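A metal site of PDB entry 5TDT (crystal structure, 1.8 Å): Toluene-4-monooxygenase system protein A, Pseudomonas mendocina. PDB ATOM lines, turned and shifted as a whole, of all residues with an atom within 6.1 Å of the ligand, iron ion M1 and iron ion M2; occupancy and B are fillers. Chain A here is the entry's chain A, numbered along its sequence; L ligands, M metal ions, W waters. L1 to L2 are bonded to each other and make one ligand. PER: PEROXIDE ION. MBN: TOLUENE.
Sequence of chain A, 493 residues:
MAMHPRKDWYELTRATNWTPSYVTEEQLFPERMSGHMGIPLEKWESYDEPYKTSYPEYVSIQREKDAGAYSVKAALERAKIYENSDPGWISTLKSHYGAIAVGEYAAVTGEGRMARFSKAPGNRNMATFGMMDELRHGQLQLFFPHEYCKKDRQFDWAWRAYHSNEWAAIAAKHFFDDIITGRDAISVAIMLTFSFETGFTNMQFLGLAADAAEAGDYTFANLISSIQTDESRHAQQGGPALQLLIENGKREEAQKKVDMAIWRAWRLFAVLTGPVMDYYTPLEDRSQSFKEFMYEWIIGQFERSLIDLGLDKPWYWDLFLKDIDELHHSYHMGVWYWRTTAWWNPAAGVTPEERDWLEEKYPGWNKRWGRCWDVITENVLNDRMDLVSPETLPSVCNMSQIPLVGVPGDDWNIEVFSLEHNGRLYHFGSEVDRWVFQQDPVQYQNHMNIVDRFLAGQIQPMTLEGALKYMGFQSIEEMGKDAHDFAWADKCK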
ATOM      1  N   ALA A  99     -29.686   4.756  -9.294  1.00  0.00           N
ATOM      2  CA  ALA A  99     -30.006   5.756 -10.303  1.00  0.00           C
ATOM      3  C   ALA A  99     -29.455   7.148  -9.981  1.00  0.00           C
ATOM      4  O   ALA A  99     -29.292   7.957 -10.905  1.00  0.00           O
ATOM      5  CB  ALA A  99     -31.528   5.828 -10.499  1.00  0.00           C
ATOM      6  N   ILE A 100     -29.136   7.442  -8.721  1.00  0.00           N
ATOM      7  CA  ILE A 100     -28.907   8.810  -8.267  1.00  0.00           C
ATOM      8  C   ILE A 100     -27.456   9.065  -7.857  1.00  0.00           C
ATOM      9  O   ILE A 100     -26.919  10.124  -8.177  1.00  0.00           O
ATOM     10  CB  ILE A 100     -29.889   9.162  -7.125  1.00  0.00           C
ATOM     11  CG1 ILE A 100     -31.340   9.201  -7.628  1.00  0.00           C
ATOM     12  CG2 ILE A 100     -29.509  10.497  -6.459  1.00  0.00           C
ATOM     13  CD1 ILE A 100     -31.584  10.157  -8.780  1.00  0.00           C
ATOM     14  N   ALA A 101     -26.832   8.138  -7.136  1.00  0.00           N
ATOM     15  CA  ALA A 101     -25.616   8.483  -6.377  1.00  0.00           C
ATOM     16  C   ALA A 101     -24.492   9.005  -7.278  1.00  0.00           C
ATOM     17  O   ALA A 101     -23.909  10.063  -7.018  1.00  0.00           O
ATOM     18  CB  ALA A 101     -25.135   7.290  -5.556  1.00  0.00           C
ATOM     19  N   VAL A 102     -24.158   8.269  -8.337  1.00  0.00           N
ATOM     20  CA  VAL A 102     -23.053   8.717  -9.170  1.00  0.00           C
ATOM     21  C   VAL A 102     -23.496   9.806 -10.140  1.00  0.00           C
ATOM     22  O   VAL A 102     -22.664  10.578 -10.615  1.00  0.00           O
ATOM     23  CB  VAL A 102     -22.422   7.473  -9.850  1.00  0.00           C
ATOM     24  CG1 VAL A 102     -21.298   7.855 -10.875  1.00  0.00           C
ATOM     25  CG2 VAL A 102     -21.862   6.550  -8.766  1.00  0.00           C
ATOM     26  N   GLY A 103     -24.803   9.939 -10.391  1.00  0.00           N
ATOM     27  CA  GLY A 103     -25.304  11.087 -11.137  1.00  0.00           C
ATOM     28  C   GLY A 103     -25.195  12.379 -10.356  1.00  0.00           C
ATOM     29  O   GLY A 103     -24.963  13.445 -10.926  1.00  0.00           O
ATOM     30  N   GLU A 104     -25.372  12.309  -9.032  1.00  0.00           N
ATOM     31  CA  GLU A 104     -25.074  13.465  -8.186  1.00  0.00           C
ATOM     32  C   GLU A 104     -23.621  13.881  -8.326  1.00  0.00           C
ATOM     33  O   GLU A 104     -23.301  15.070  -8.415  1.00  0.00           O
ATOM     34  CB  GLU A 104     -25.378  13.137  -6.724  1.00  0.00           C
ATOM     35  CG  GLU A 104     -26.823  12.826  -6.475  1.00  0.00           C
ATOM     36  CD  GLU A 104     -27.573  13.985  -5.866  1.00  0.00           C
ATOM     37  OE1 GLU A 104     -28.544  13.726  -5.128  1.00  0.00           O
ATOM     38  OE2 GLU A 104     -27.177  15.159  -6.105  1.00  0.00           O
ATOM     39  N   ALA A 107     -23.115  15.839 -11.300  1.00  0.00           N
ATOM     40  CA  ALA A 107     -23.592  17.213 -11.199  1.00  0.00           C
ATOM     41  C   ALA A 107     -22.506  18.171 -10.722  1.00  0.00           C
ATOM     42  O   ALA A 107     -22.595  19.377 -10.993  1.00  0.00           O
ATOM     43  CB  ALA A 107     -24.813  17.290 -10.271  1.00  0.00           C
ATOM     44  N   GLU A 111     -21.922  22.049 -12.255  1.00  0.00           N
ATOM     45  CA  GLU A 111     -21.632  23.233 -11.467  1.00  0.00           C
ATOM     46  C   GLU A 111     -20.235  23.782 -11.779  1.00  0.00           C
ATOM     47  O   GLU A 111     -20.035  24.990 -11.865  1.00  0.00           O
ATOM     48  CB  GLU A 111     -21.752  22.902  -9.965  1.00  0.00           C
ATOM     49  CG  GLU A 111     -23.186  22.539  -9.489  1.00  0.00           C
ATOM     50  CD  GLU A 111     -24.140  23.736  -9.396  1.00  0.00           C
ATOM     51  OE1 GLU A 111     -23.687  24.896  -9.516  1.00  0.00           O
ATOM     52  OE2 GLU A 111     -25.368  23.511  -9.173  1.00  0.00           O
ATOM     53  N   ASP A 133     -21.936  21.243  -2.853  1.00  0.00           N
ATOM     54  CA  ASP A 133     -23.198  20.560  -2.538  1.00  0.00           C
ATOM     55  C   ASP A 133     -23.267  19.204  -3.224  1.00  0.00           C
ATOM     56  O   ASP A 133     -23.670  18.202  -2.605  1.00  0.00           O
ATOM     57  CB  ASP A 133     -24.397  21.412  -2.961  1.00  0.00           C
ATOM     58  CG  ASP A 133     -24.557  22.685  -2.157  1.00  0.00           C
ATOM     59  OD1 ASP A 133     -23.972  22.834  -1.044  1.00  0.00           O
ATOM     60  OD2 ASP A 133     -25.307  23.552  -2.642  1.00  0.00           O
ATOM     61  N   GLU A 134     -22.934  19.143  -4.515  1.00  0.00           N
ATOM     62  CA  GLU A 134     -23.131  17.870  -5.204  1.00  0.00           C
ATOM     63  C   GLU A 134     -22.064  16.854  -4.791  1.00  0.00           C
ATOM     64  O   GLU A 134     -22.323  15.647  -4.817  1.00  0.00           O
ATOM     65  CB  GLU A 134     -23.144  18.065  -6.722  1.00  0.00           C
ATOM     66  CG  GLU A 134     -24.164  19.102  -7.215  1.00  0.00           C
ATOM     67  CD  GLU A 134     -25.633  18.693  -7.020  1.00  0.00           C
ATOM     68  OE1 GLU A 134     -25.952  17.746  -6.250  1.00  0.00           O
ATOM     69  OE2 GLU A 134     -26.493  19.337  -7.664  1.00  0.00           O
ATOM     70  N   HIS A 137     -23.696  15.325  -1.903  1.00  0.00           N
ATOM     71  CA  HIS A 137     -24.796  14.434  -2.244  1.00  0.00           C
ATOM     72  C   HIS A 137     -24.296  13.108  -2.811  1.00  0.00           C
ATOM     73  O   HIS A 137     -24.850  12.052  -2.492  1.00  0.00           O
ATOM     74  CB  HIS A 137     -25.747  15.123  -3.223  1.00  0.00           C
ATOM     75  CG  HIS A 137     -26.310  16.403  -2.693  1.00  0.00           C
ATOM     76  ND1 HIS A 137     -27.003  17.306  -3.470  1.00  0.00           N
ATOM     77  CD2 HIS A 137     -26.280  16.928  -1.440  1.00  0.00           C
ATOM     78  CE1 HIS A 137     -27.369  18.338  -2.728  1.00  0.00           C
ATOM     79  NE2 HIS A 137     -26.943  18.135  -1.483  1.00  0.00           N
ATOM     80  N   GLN A 141     -24.734   9.527  -0.723  1.00  0.00           N
ATOM     81  CA  GLN A 141     -25.541   8.479  -1.331  1.00  0.00           C
ATOM     82  C   GLN A 141     -24.713   7.298  -1.812  1.00  0.00           C
ATOM     83  O   GLN A 141     -25.290   6.320  -2.304  1.00  0.00           O
ATOM     84  CB  GLN A 141     -26.394   9.086  -2.437  1.00  0.00           C
ATOM     85  CG  GLN A 141     -27.520   9.861  -1.768  1.00  0.00           C
ATOM     86  CD  GLN A 141     -28.341  10.684  -2.702  1.00  0.00           C
ATOM     87  OE1 GLN A 141     -29.559  10.475  -2.812  1.00  0.00           O
ATOM     88  NE2 GLN A 141     -27.717  11.655  -3.350  1.00  0.00           N
ATOM     89  N   TYR A 162     -23.755   3.423 -12.941  1.00  0.00           N
ATOM     90  CA  TYR A 162     -23.324   4.374 -13.964  1.00  0.00           C
ATOM     91  C   TYR A 162     -22.094   3.888 -14.723  1.00  0.00           C
ATOM     92  O   TYR A 162     -21.750   4.449 -15.763  1.00  0.00           O
ATOM     93  CB  TYR A 162     -23.039   5.751 -13.334  1.00  0.00           C
ATOM     94  CG  TYR A 162     -24.283   6.632 -13.157  1.00  0.00           C
ATOM     95  CD1 TYR A 162     -25.281   6.267 -12.261  1.00  0.00           C
ATOM     96  CD2 TYR A 162     -24.429   7.819 -13.867  1.00  0.00           C
ATOM     97  CE1 TYR A 162     -26.427   7.066 -12.090  1.00  0.00           C
ATOM     98  CE2 TYR A 162     -25.554   8.639 -13.694  1.00  0.00           C
ATOM     99  CZ  TYR A 162     -26.543   8.252 -12.805  1.00  0.00           C
ATOM    100  OH  TYR A 162     -27.666   9.043 -12.639  1.00  0.00           O
ATOM    101  N   PHE A 176     -28.569  12.761 -18.117  1.00  0.00           N
ATOM    102  CA  PHE A 176     -27.677  13.606 -17.334  1.00  0.00           C
ATOM    103  C   PHE A 176     -26.483  14.105 -18.144  1.00  0.00           C
ATOM    104  O   PHE A 176     -26.030  15.239 -17.930  1.00  0.00           O
ATOM    105  CB  PHE A 176     -27.199  12.885 -16.075  1.00  0.00           C
ATOM    106  CG  PHE A 176     -28.267  12.700 -15.040  1.00  0.00           C
ATOM    107  CD1 PHE A 176     -29.093  13.765 -14.668  1.00  0.00           C
ATOM    108  CD2 PHE A 176     -28.503  11.470 -14.474  1.00  0.00           C
ATOM    109  CE1 PHE A 176     -30.097  13.598 -13.725  1.00  0.00           C
ATOM    110  CE2 PHE A 176     -29.501  11.298 -13.538  1.00  0.00           C
ATOM    111  CZ  PHE A 176     -30.304  12.355 -13.172  1.00  0.00           C
ATOM    112  N   ILE A 180     -26.508  17.981 -17.946  1.00  0.00           N
ATOM    113  CA  ILE A 180     -25.550  18.348 -16.898  1.00  0.00           C
ATOM    114  C   ILE A 180     -24.136  18.544 -17.467  1.00  0.00           C
ATOM    115  O   ILE A 180     -23.536  19.611 -17.304  1.00  0.00           O
ATOM    116  CB  ILE A 180     -25.537  17.322 -15.742  1.00  0.00           C
ATOM    117  CG1 ILE A 180     -26.903  17.263 -15.067  1.00  0.00           C
ATOM    118  CG2 ILE A 180     -24.422  17.683 -14.751  1.00  0.00           C
ATOM    119  CD1 ILE A 180     -26.945  16.356 -13.863  1.00  0.00           C
ATOM    120  N   LEU A 192     -30.376  22.301 -15.965  1.00  0.00           N
ATOM    121  CA  LEU A 192     -30.141  21.606 -14.694  1.00  0.00           C
ATOM    122  C   LEU A 192     -30.764  22.391 -13.542  1.00  0.00           C
ATOM    123  O   LEU A 192     -31.732  21.934 -12.930  1.00  0.00           O
ATOM    124  CB  LEU A 192     -28.645  21.401 -14.468  1.00  0.00           C
ATOM    125  CG  LEU A 192     -28.242  20.906 -13.062  1.00  0.00           C
ATOM    126  CD1 LEU A 192     -28.878  19.547 -12.731  1.00  0.00           C
ATOM    127  CD2 LEU A 192     -26.729  20.821 -12.924  1.00  0.00           C
ATOM    128  N   PHE A 196     -34.621  20.960 -13.974  1.00  0.00           N
ATOM    129  CA  PHE A 196     -34.554  19.706 -13.237  1.00  0.00           C
ATOM    130  C   PHE A 196     -34.579  19.943 -11.720  1.00  0.00           C
ATOM    131  O   PHE A 196     -35.313  19.268 -10.991  1.00  0.00           O
ATOM    132  CB  PHE A 196     -33.296  18.952 -13.645  1.00  0.00           C
ATOM    133  CG  PHE A 196     -33.140  17.609 -13.008  1.00  0.00           C
ATOM    134  CD1 PHE A 196     -34.091  16.616 -13.238  1.00  0.00           C
ATOM    135  CD2 PHE A 196     -32.046  17.323 -12.212  1.00  0.00           C
ATOM    136  CE1 PHE A 196     -33.946  15.359 -12.644  1.00  0.00           C
ATOM    137  CE2 PHE A 196     -31.903  16.084 -11.631  1.00  0.00           C
ATOM    138  CZ  PHE A 196     -32.848  15.097 -11.847  1.00  0.00           C
ATOM    139  N   GLU A 197     -33.807  20.927 -11.230  1.00  0.00           N
ATOM    140  CA  GLU A 197     -33.556  21.043  -9.796  1.00  0.00           C
ATOM    141  C   GLU A 197     -34.621  21.846  -9.035  1.00  0.00           C
ATOM    142  O   GLU A 197     -34.744  21.652  -7.815  1.00  0.00           O
ATOM    143  CB  GLU A 197     -32.181  21.643  -9.534  1.00  0.00           C
ATOM    144  CG  GLU A 197     -31.045  20.686  -9.944  1.00  0.00           C
ATOM    145  CD  GLU A 197     -29.652  21.153  -9.541  1.00  0.00           C
ATOM    146  OE1 GLU A 197     -29.332  22.348  -9.680  1.00  0.00           O
ATOM    147  OE2 GLU A 197     -28.860  20.317  -9.072  1.00  0.00           O
ATOM    148  N   THR A 201     -36.712  17.166  -9.110  1.00  0.00           N
ATOM    149  CA  THR A 201     -36.084  16.443  -8.007  1.00  0.00           C
ATOM    150  C   THR A 201     -36.942  16.447  -6.748  1.00  0.00           C
ATOM    151  O   THR A 201     -36.812  15.555  -5.904  1.00  0.00           O
ATOM    152  CB  THR A 201     -34.694  16.992  -7.681  1.00  0.00           C
ATOM    153  OG1 THR A 201     -34.791  18.392  -7.394  1.00  0.00           O
ATOM    154  CG2 THR A 201     -33.734  16.766  -8.858  1.00  0.00           C
ATOM    155  N   PHE A 205     -36.989  13.399  -3.990  1.00  0.00           N
ATOM    156  CA  PHE A 205     -36.338  13.676  -2.719  1.00  0.00           C
ATOM    157  C   PHE A 205     -37.281  14.164  -1.627  1.00  0.00           C
ATOM    158  O   PHE A 205     -36.871  14.211  -0.456  1.00  0.00           O
ATOM    159  CB  PHE A 205     -35.213  14.703  -2.905  1.00  0.00           C
ATOM    160  CG  PHE A 205     -33.999  14.138  -3.575  1.00  0.00           C
ATOM    161  CD1 PHE A 205     -33.984  13.950  -4.956  1.00  0.00           C
ATOM    162  CD2 PHE A 205     -32.887  13.784  -2.835  1.00  0.00           C
ATOM    163  CE1 PHE A 205     -32.848  13.429  -5.590  1.00  0.00           C
ATOM    164  CE2 PHE A 205     -31.760  13.255  -3.456  1.00  0.00           C
ATOM    165  CZ  PHE A 205     -31.749  13.073  -4.845  1.00  0.00           C
ATOM    166  N   ILE A 227     -30.668  16.566   1.897  1.00  0.00           N
ATOM    167  CA  ILE A 227     -30.062  16.829   0.605  1.00  0.00           C
ATOM    168  C   ILE A 227     -30.853  17.908  -0.128  1.00  0.00           C
ATOM    169  O   ILE A 227     -30.288  18.845  -0.711  1.00  0.00           O
ATOM    170  CB  ILE A 227     -29.986  15.512  -0.194  1.00  0.00           C
ATOM    171  CG1 ILE A 227     -28.849  14.648   0.365  1.00  0.00           C
ATOM    172  CG2 ILE A 227     -29.847  15.781  -1.695  1.00  0.00           C
ATOM    173  CD1 ILE A 227     -28.814  13.233  -0.220  1.00  0.00           C
ATOM    174  N   ASP A 230     -30.054  21.635   0.296  1.00  0.00           N
ATOM    175  CA  ASP A 230     -28.999  22.192  -0.555  1.00  0.00           C
ATOM    176  C   ASP A 230     -29.537  22.522  -1.942  1.00  0.00           C
ATOM    177  O   ASP A 230     -29.230  23.583  -2.505  1.00  0.00           O
ATOM    178  CB  ASP A 230     -27.812  21.207  -0.690  1.00  0.00           C
ATOM    179  CG  ASP A 230     -27.177  20.829   0.649  1.00  0.00           C
ATOM    180  OD1 ASP A 230     -26.793  19.659   0.786  1.00  0.00           O
ATOM    181  OD2 ASP A 230     -27.056  21.701   1.549  1.00  0.00           O
ATOM    182  N   GLU A 231     -30.259  21.572  -2.533  1.00  0.00           N
ATOM    183  CA  GLU A 231     -30.861  21.773  -3.852  1.00  0.00           C
ATOM    184  C   GLU A 231     -31.630  23.085  -3.895  1.00  0.00           C
ATOM    185  O   GLU A 231     -31.491  23.867  -4.850  1.00  0.00           O
ATOM    186  CB  GLU A 231     -31.782  20.592  -4.176  1.00  0.00           C
ATOM    187  CG  GLU A 231     -32.439  20.684  -5.538  1.00  0.00           C
ATOM    188  CD  GLU A 231     -31.622  20.010  -6.619  1.00  0.00           C
ATOM    189  OE1 GLU A 231     -32.141  19.078  -7.275  1.00  0.00           O
ATOM    190  OE2 GLU A 231     -30.458  20.405  -6.795  1.00  0.00           O
ATOM    191  N   HIS A 234     -28.953  26.014  -4.366  1.00  0.00           N
ATOM    192  CA  HIS A 234     -28.182  26.206  -5.601  1.00  0.00           C
ATOM    193  C   HIS A 234     -29.047  26.097  -6.861  1.00  0.00           C
ATOM    194  O   HIS A 234     -28.616  26.573  -7.916  1.00  0.00           O
ATOM    195  CB  HIS A 234     -26.965  25.256  -5.676  1.00  0.00           C
ATOM    196  CG  HIS A 234     -27.291  23.803  -5.807  1.00  0.00           C
ATOM    197  ND1 HIS A 234     -26.847  22.861  -4.898  1.00  0.00           N
ATOM    198  CD2 HIS A 234     -27.941  23.108  -6.776  1.00  0.00           C
ATOM    199  CE1 HIS A 234     -27.250  21.655  -5.272  1.00  0.00           C
ATOM    200  NE2 HIS A 234     -27.915  21.785  -6.414  1.00  0.00           N
ATOM    201  N   ALA A 235     -30.260  25.547  -6.765  1.00  0.00           N
ATOM    202  CA  ALA A 235     -31.178  25.615  -7.897  1.00  0.00           C
ATOM    203  C   ALA A 235     -31.599  27.055  -8.216  1.00  0.00           C
ATOM    204  O   ALA A 235     -32.013  27.330  -9.337  1.00  0.00           O
ATOM    205  CB  ALA A 235     -32.432  24.764  -7.649  1.00  0.00           C
HETATM  206  O1  PER L   1     -29.160  17.064  -7.687  1.00  0.00           O
HETATM  207  O2  PER L   1     -27.900  17.368  -8.239  1.00  0.00           O
HETATM  208  C   MBN L   2     -28.939  12.347 -10.111  1.00  0.00           C
HETATM  209  C1  MBN L   2     -29.126  13.789  -9.675  1.00  0.00           C
HETATM  210  C2  MBN L   2     -28.342  14.764 -10.264  1.00  0.00           C
HETATM  211  C3  MBN L   2     -28.509  16.081  -9.886  1.00  0.00           C
HETATM  212  C4  MBN L   2     -29.414  16.429  -8.886  1.00  0.00           C
HETATM  213  C5  MBN L   2     -30.194  15.437  -8.296  1.00  0.00           C
HETATM  214  C6  MBN L   2     -30.050  14.116  -8.691  1.00  0.00           C
HETATM  215 FE    FE M   1     -27.771  17.061  -5.569  1.00  0.00          FE
HETATM  216 FE    FE M   2     -28.532  19.758  -7.234  1.00  0.00          FE
HETATM  217  O   HOH W   1     -28.794  18.938  -5.531  1.00  0.00           O
HETATM  218  O   HOH W   2     -29.465  16.193  -4.860  1.00  0.00           O
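The backbone carbonyl oxygen of Glu 197 is in hydrogen-bond range of the side-chain hydroxyl of Thr 201. N of Glu 197 sits at hydrogen-bond distance from O of Leu 192 (2.9 Å). OE1 of Glu 104 lies within hydrogen-bond range of NE2 of Gln 141 (2.9 Å). The side-chain carboxylate (OE1) of Glu 231 is in hydrogen-bond range of the side-chain hydroxyl (OG1) of Thr 201. A ring nitrogen (NE2) of His 137 sits close to the backbone carbonyl oxygen (O) of Asp 133, 3.5 Å away. A ring nitrogen (ND1) of His 234 sits at hydrogen-bond distance from the side-chain carboxylate of Asp 133, at 2.8 Å. ND1 of His 234 sits at hydrogen-bond distance from O of Asp 230 (3.5 Å). O of Phe 196 sits at hydrogen-bond distance from N of Thr 201, 3.1 Å away.
O of Ile 100 touches C of MBN L2, at 3.6 Å. Gly 103 touches the ligand. Ala 107 touches the ligand. CZ of Phe 176 touches C of MBN L2, 3.4 Å away. CE2 of Phe 196 touches C4 of MBN L2, 3.7 Å away. CG2 of Thr 201 touches C5 of MBN L2, 3.8 Å away. Hydrophobic or aromatic side chains that line the ligand: Ile 100, Ala 107, Phe 176 and Phe 196. The nearest printed residue that does not touch the ligand is Ile 180 (4.2 Å).
Three residues have an atom within 4 Å of iron ion M1: Glu 104, Glu 134 and His 137.
The nearest printed residue that does not touch iron ion M2 is His 137 (4.7 Å).
Iron ion M1 is bound by water W2 (2.0 Å), OE1 of Glu 134 (2.1 Å), OE2 of Glu 104 (2.1 Å), water W1 (2.1 Å), ND1 of His 137 (2.2 Å) and O1 of PER L1 (2.5 Å). Iron ion M1 has six donor atoms within binding distance.
Iron ion M2 is bound by water W1 (1.9 Å), OE2 of Glu 197 (1.9 Å), OE2 of Glu 231 (2.1 Å), OE2 of Glu 134 (2.1 Å) and NE2 of His 234 (2.3 Å). Iron ion M2 has five donor atoms within binding distance. Slightly farther from iron ion M2 lies O2 of PER L1 (2.7 Å).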
